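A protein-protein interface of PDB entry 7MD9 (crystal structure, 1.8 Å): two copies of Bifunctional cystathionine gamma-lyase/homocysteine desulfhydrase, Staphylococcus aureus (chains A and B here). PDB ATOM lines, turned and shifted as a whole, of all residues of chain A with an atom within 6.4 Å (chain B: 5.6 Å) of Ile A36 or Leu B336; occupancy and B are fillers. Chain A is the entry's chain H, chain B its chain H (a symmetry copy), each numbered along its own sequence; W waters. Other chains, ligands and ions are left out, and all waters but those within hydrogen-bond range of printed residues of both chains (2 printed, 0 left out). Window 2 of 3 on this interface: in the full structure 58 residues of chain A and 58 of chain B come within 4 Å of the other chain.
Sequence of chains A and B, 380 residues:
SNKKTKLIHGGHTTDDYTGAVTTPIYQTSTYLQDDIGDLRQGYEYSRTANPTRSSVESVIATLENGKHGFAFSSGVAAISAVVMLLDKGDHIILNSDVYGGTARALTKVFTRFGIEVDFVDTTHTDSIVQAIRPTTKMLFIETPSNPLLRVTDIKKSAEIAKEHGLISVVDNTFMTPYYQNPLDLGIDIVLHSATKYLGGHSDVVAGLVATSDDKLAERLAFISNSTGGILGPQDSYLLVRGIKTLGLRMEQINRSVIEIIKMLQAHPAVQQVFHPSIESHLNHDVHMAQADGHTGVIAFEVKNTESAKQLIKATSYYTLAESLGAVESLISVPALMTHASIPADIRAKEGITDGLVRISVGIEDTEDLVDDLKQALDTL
Water W2 lies within hydrogen-bond range of the side-chain amino group (NZ) of Lys B309 (2.4 Å) and the backbone carbonyl oxygen (O) of Ile A36 (2.7 Å). Water W1 bridges the side-chain amino group (NZ) of Lys B309 and the backbone NH (N) of Ile A36.
SD of Met B337 is in hydrogen-bond range of N of Val B333, 3.5 Å away. The side-chain amide oxygen (OE1) of Gln A33 lies within hydrogen-bond range of the backbone NH (N) of Gly A37, at 2.9 Å.
Ile A36 touches just these residues of chain B: Ile B312 (3.97 Å), Leu B320 (3.7 Å), Val B333 (3.6 Å), Leu B336 (3.8 Å) and Met B337 (3.8 Å). Leu B336 touches one residue of chain A. Of the printed residues of chain A, Met B337 touches Ile A36 (3.8 Å). Printed residues of chain B within 4 Å of Asp A35: Leu B320 (3.8 Å). Of the printed residues of chain B, Gln A33 touches Leu B320 (3.1 Å). Printed residues of chain A within 4 Å of Val B333: Ile A36. Printed residues of chain A within 4 Å of Ile B312: Ile A36 (3.97 Å). Ala B340 touches none of the printed residues of chain A. The nearest residue of chain B that does not touch Ile A36 is Lys B309 (4.3 Å). The nearest residue of chain A that does not touch Leu B336 is Gly A37 (6.3 Å).
The backbone NH (N) of Gln A33 lies within hydrogen-bond range of the backbone carbonyl oxygen (O) of Leu B320 (3.1 Å).
Among the printed residues, merely in contact across the chains: Ile A36 with Val B333, Ile A36 with Leu B320, Asp A35 with Leu B320, Ile A36 with Met B337, Ile A36 with Leu B336 and Ile A36 with Ile B312.
Printed residues of chain A that touch a printed residue of chain B: Gln A33, Asp A35 and Ile A36. Hydrophobic or aromatic side chains of chain A that line the printed part of chain B: Ile A36. Of the 12 printed residues of chain B, 5 touch a printed residue of chain A. Hydrophobic or aromatic side chains of chain B within 4 Å of the printed part of chain A: Ile B312, Leu B320, Val B333, Leu B336 and Met B337. Among the printed residues, 7 pairs touch across the chains.
No position is printed for both chains. Of the 7 pairs that touch across the chains among the printed residues, none has its exchanged pair printed and touching as well.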
ATOM      1  N   GLN A  33      30.231  22.902 -19.332  1.00  0.00           N
ATOM      2  CA  GLN A  33      30.643  22.278 -20.582  1.00  0.00           C
ATOM      3  C   GLN A  33      31.794  23.089 -21.170  1.00  0.00           C
ATOM      4  O   GLN A  33      31.694  24.313 -21.295  1.00  0.00           O
ATOM      5  CB  GLN A  33      29.478  22.200 -21.567  1.00  0.00           C
ATOM      6  CG  GLN A  33      28.264  21.427 -21.031  1.00  0.00           C
ATOM      7  CD  GLN A  33      27.112  21.391 -22.012  1.00  0.00           C
ATOM      8  OE1 GLN A  33      27.318  21.455 -23.225  1.00  0.00           O
ATOM      9  NE2 GLN A  33      25.883  21.293 -21.494  1.00  0.00           N
ATOM     10  N   ASP A  34      32.894  22.412 -21.501  1.00  0.00           N
ATOM     11  CA  ASP A  34      34.049  23.129 -22.037  1.00  0.00           C
ATOM     12  C   ASP A  34      33.804  23.584 -23.471  1.00  0.00           C
ATOM     13  O   ASP A  34      34.276  24.650 -23.877  1.00  0.00           O
ATOM     14  CB  ASP A  34      35.292  22.248 -21.933  1.00  0.00           C
ATOM     15  CG  ASP A  34      35.706  22.009 -20.486  1.00  0.00           C
ATOM     16  OD1 ASP A  34      35.596  22.960 -19.683  1.00  0.00           O
ATOM     17  OD2 ASP A  34      36.115  20.878 -20.149  1.00  0.00           O
ATOM     18  N   ASP A  35      33.066  22.794 -24.238  1.00  0.00           N
ATOM     19  CA  ASP A  35      32.524  23.183 -25.529  1.00  0.00           C
ATOM     20  C   ASP A  35      31.092  22.688 -25.570  1.00  0.00           C
ATOM     21  O   ASP A  35      30.721  21.781 -24.823  1.00  0.00           O
ATOM     22  CB  ASP A  35      33.316  22.588 -26.704  1.00  0.00           C
ATOM     23  CG  ASP A  35      34.750  23.071 -26.746  1.00  0.00           C
ATOM     24  OD1 ASP A  35      34.994  24.162 -27.304  1.00  0.00           O
ATOM     25  OD2 ASP A  35      35.631  22.357 -26.218  1.00  0.00           O
ATOM     26  N   ILE A  36      30.289  23.281 -26.453  1.00  0.00           N
ATOM     27  CA  ILE A  36      28.883  22.901 -26.534  1.00  0.00           C
ATOM     28  C   ILE A  36      28.778  21.412 -26.825  1.00  0.00           C
ATOM     29  O   ILE A  36      29.267  20.927 -27.854  1.00  0.00           O
ATOM     30  CB  ILE A  36      28.156  23.725 -27.593  1.00  0.00           C
ATOM     31  CG1 ILE A  36      28.012  25.167 -27.126  1.00  0.00           C
ATOM     32  CG2 ILE A  36      26.792  23.113 -27.881  1.00  0.00           C
ATOM     33  CD1 ILE A  36      27.322  26.049 -28.124  1.00  0.00           C
ATOM     34  N   GLY A  37      28.147  20.677 -25.907  1.00  0.00           N
ATOM     35  CA  GLY A  37      27.922  19.260 -26.066  1.00  0.00           C
ATOM     36  C   GLY A  37      29.037  18.372 -25.562  1.00  0.00           C
ATOM     37  O   GLY A  37      28.867  17.146 -25.533  1.00  0.00           O
ATOM     38  N   ASP A  38      30.173  18.938 -25.169  1.00  0.00           N
ATOM     39  CA  ASP A  38      31.280  18.147 -24.652  1.00  0.00           C
ATOM     40  C   ASP A  38      31.218  18.168 -23.131  1.00  0.00           C
ATOM     41  O   ASP A  38      31.473  19.200 -22.501  1.00  0.00           O
ATOM     42  CB  ASP A  38      32.618  18.669 -25.168  1.00  0.00           C
ATOM     43  CG  ASP A  38      32.800  18.418 -26.657  1.00  0.00           C
ATOM     44  OD1 ASP A  38      31.889  17.822 -27.276  1.00  0.00           O
ATOM     45  OD2 ASP A  38      33.861  18.799 -27.203  1.00  0.00           O
ATOM     46  N   THR B 305      25.973  30.102 -36.067  1.00  0.00           N
ATOM     47  CA  THR B 305      26.552  29.209 -35.067  1.00  0.00           C
ATOM     48  C   THR B 305      27.973  29.618 -34.721  1.00  0.00           C
ATOM     49  O   THR B 305      28.376  29.576 -33.551  1.00  0.00           O
ATOM     50  CB  THR B 305      26.543  27.767 -35.579  1.00  0.00           C
ATOM     51  OG1 THR B 305      25.195  27.348 -35.823  1.00  0.00           O
ATOM     52  CG2 THR B 305      27.196  26.835 -34.566  1.00  0.00           C
ATOM     53  N   LYS B 309      29.211  30.516 -30.908  1.00  0.00           N
ATOM     54  CA  LYS B 309      30.303  29.846 -30.211  1.00  0.00           C
ATOM     55  C   LYS B 309      31.402  30.835 -29.840  1.00  0.00           C
ATOM     56  O   LYS B 309      31.973  30.756 -28.745  1.00  0.00           O
ATOM     57  CB  LYS B 309      30.864  28.717 -31.075  1.00  0.00           C
ATOM     58  CG  LYS B 309      29.975  27.475 -31.148  1.00  0.00           C
ATOM     59  CD  LYS B 309      30.619  26.393 -32.013  1.00  0.00           C
ATOM     60  CE  LYS B 309      30.214  24.991 -31.572  1.00  0.00           C
ATOM     61  NZ  LYS B 309      31.352  24.319 -30.857  1.00  0.00           N
ATOM     62  N   ILE B 312      30.441  32.920 -26.754  1.00  0.00           N
ATOM     63  CA  ILE B 312      30.580  32.163 -25.514  1.00  0.00           C
ATOM     64  C   ILE B 312      32.038  32.102 -25.083  1.00  0.00           C
ATOM     65  O   ILE B 312      32.364  32.309 -23.906  1.00  0.00           O
ATOM     66  CB  ILE B 312      29.984  30.756 -25.687  1.00  0.00           C
ATOM     67  CG1 ILE B 312      28.467  30.847 -25.831  1.00  0.00           C
ATOM     68  CG2 ILE B 312      30.387  29.854 -24.522  1.00  0.00           C
ATOM     69  CD1 ILE B 312      27.833  29.584 -26.390  1.00  0.00           C
ATOM     70  N   LEU B 320      28.888  28.500 -19.699  1.00  0.00           N
ATOM     71  CA  LEU B 320      28.199  27.576 -20.598  1.00  0.00           C
ATOM     72  C   LEU B 320      27.755  26.354 -19.805  1.00  0.00           C
ATOM     73  O   LEU B 320      28.585  25.529 -19.398  1.00  0.00           O
ATOM     74  CB  LEU B 320      29.108  27.170 -21.757  1.00  0.00           C
ATOM     75  CG  LEU B 320      28.534  26.096 -22.684  1.00  0.00           C
ATOM     76  CD1 LEU B 320      27.285  26.618 -23.386  1.00  0.00           C
ATOM     77  CD2 LEU B 320      29.584  25.629 -23.695  1.00  0.00           C
ATOM     78  N   VAL B 333      23.014  27.882 -26.315  1.00  0.00           N
ATOM     79  CA  VAL B 333      22.574  28.011 -27.705  1.00  0.00           C
ATOM     80  C   VAL B 333      21.452  27.005 -27.942  1.00  0.00           C
ATOM     81  O   VAL B 333      21.727  25.815 -28.149  1.00  0.00           O
ATOM     82  CB  VAL B 333      23.732  27.786 -28.693  1.00  0.00           C
ATOM     83  CG1 VAL B 333      23.264  28.047 -30.131  1.00  0.00           C
ATOM     84  CG2 VAL B 333      24.913  28.688 -28.357  1.00  0.00           C
ATOM     85  N   PRO B 334      20.189  27.438 -27.894  1.00  0.00           N
ATOM     86  CA  PRO B 334      19.067  26.486 -27.981  1.00  0.00           C
ATOM     87  C   PRO B 334      19.114  25.560 -29.180  1.00  0.00           C
ATOM     88  O   PRO B 334      18.820  24.365 -29.037  1.00  0.00           O
ATOM     89  CB  PRO B 334      17.847  27.414 -28.041  1.00  0.00           C
ATOM     90  CG  PRO B 334      18.276  28.608 -27.247  1.00  0.00           C
ATOM     91  CD  PRO B 334      19.738  28.797 -27.553  1.00  0.00           C
ATOM     92  N   ALA B 335      19.479  26.074 -30.361  1.00  0.00           N
ATOM     93  CA  ALA B 335      19.474  25.231 -31.552  1.00  0.00           C
ATOM     94  C   ALA B 335      20.404  24.040 -31.395  1.00  0.00           C
ATOM     95  O   ALA B 335      20.151  22.981 -31.977  1.00  0.00           O
ATOM     96  CB  ALA B 335      19.855  26.046 -32.789  1.00  0.00           C
ATOM     97  N   LEU B 336      21.462  24.174 -30.595  1.00  0.00           N
ATOM     98  CA  LEU B 336      22.396  23.077 -30.391  1.00  0.00           C
ATOM     99  C   LEU B 336      22.167  22.306 -29.102  1.00  0.00           C
ATOM    100  O   LEU B 336      22.634  21.168 -28.989  1.00  0.00           O
ATOM    101  CB  LEU B 336      23.839  23.598 -30.382  1.00  0.00           C
ATOM    102  CG  LEU B 336      24.331  24.253 -31.668  1.00  0.00           C
ATOM    103  CD1 LEU B 336      25.635  24.980 -31.405  1.00  0.00           C
ATOM    104  CD2 LEU B 336      24.499  23.193 -32.748  1.00  0.00           C
ATOM    105  N   MET B 337      21.498  22.892 -28.122  1.00  0.00           N
ATOM    106  CA  MET B 337      21.495  22.316 -26.786  1.00  0.00           C
ATOM    107  C   MET B 337      20.130  21.861 -26.306  1.00  0.00           C
ATOM    108  O   MET B 337      20.057  20.937 -25.494  1.00  0.00           O
ATOM    109  CB  MET B 337      22.065  23.319 -25.778  1.00  0.00           C
ATOM    110  CG  MET B 337      23.565  23.487 -25.909  1.00  0.00           C
ATOM    111  SD  MET B 337      24.187  24.903 -24.998  1.00  0.00           S
ATOM    112  CE  MET B 337      23.946  24.365 -23.298  1.00  0.00           C
ATOM    113  N   THR B 338      19.055  22.490 -26.762  1.00  0.00           N
ATOM    114  CA  THR B 338      17.720  22.111 -26.332  1.00  0.00           C
ATOM    115  C   THR B 338      16.771  21.809 -27.478  1.00  0.00           C
ATOM    116  O   THR B 338      15.760  21.136 -27.245  1.00  0.00           O
ATOM    117  CB  THR B 338      17.104  23.209 -25.444  1.00  0.00           C
ATOM    118  OG1 THR B 338      16.976  24.424 -26.191  1.00  0.00           O
ATOM    119  CG2 THR B 338      17.980  23.462 -24.211  1.00  0.00           C
ATOM    120  N   HIS B 339      17.070  22.244 -28.705  1.00  0.00           N
ATOM    121  CA  HIS B 339      16.199  22.016 -29.853  1.00  0.00           C
ATOM    122  C   HIS B 339      16.915  21.298 -30.992  1.00  0.00           C
ATOM    123  O   HIS B 339      16.494  21.410 -32.147  1.00  0.00           O
ATOM    124  CB  HIS B 339      15.622  23.340 -30.362  1.00  0.00           C
ATOM    125  CG  HIS B 339      14.752  24.049 -29.370  1.00  0.00           C
ATOM    126  ND1 HIS B 339      15.203  24.447 -28.128  1.00  0.00           N
ATOM    127  CD2 HIS B 339      13.455  24.434 -29.440  1.00  0.00           C
ATOM    128  CE1 HIS B 339      14.221  25.046 -27.478  1.00  0.00           C
ATOM    129  NE2 HIS B 339      13.150  25.054 -28.253  1.00  0.00           N
ATOM    130  N   ALA B 340      17.987  20.557 -30.699  1.00  0.00           N
ATOM    131  CA  ALA B 340      18.801  19.992 -31.772  1.00  0.00           C
ATOM    132  C   ALA B 340      18.119  18.833 -32.487  1.00  0.00           C
ATOM    133  O   ALA B 340      18.502  18.508 -33.616  1.00  0.00           O
ATOM    134  CB  ALA B 340      20.152  19.529 -31.228  1.00  0.00           C
HETATM  135  O   HOH W   1      31.422  25.185 -28.309  1.00  0.00           O
HETATM  136  O   HOH W   2      30.639  22.260 -29.790  1.00  0.00           O
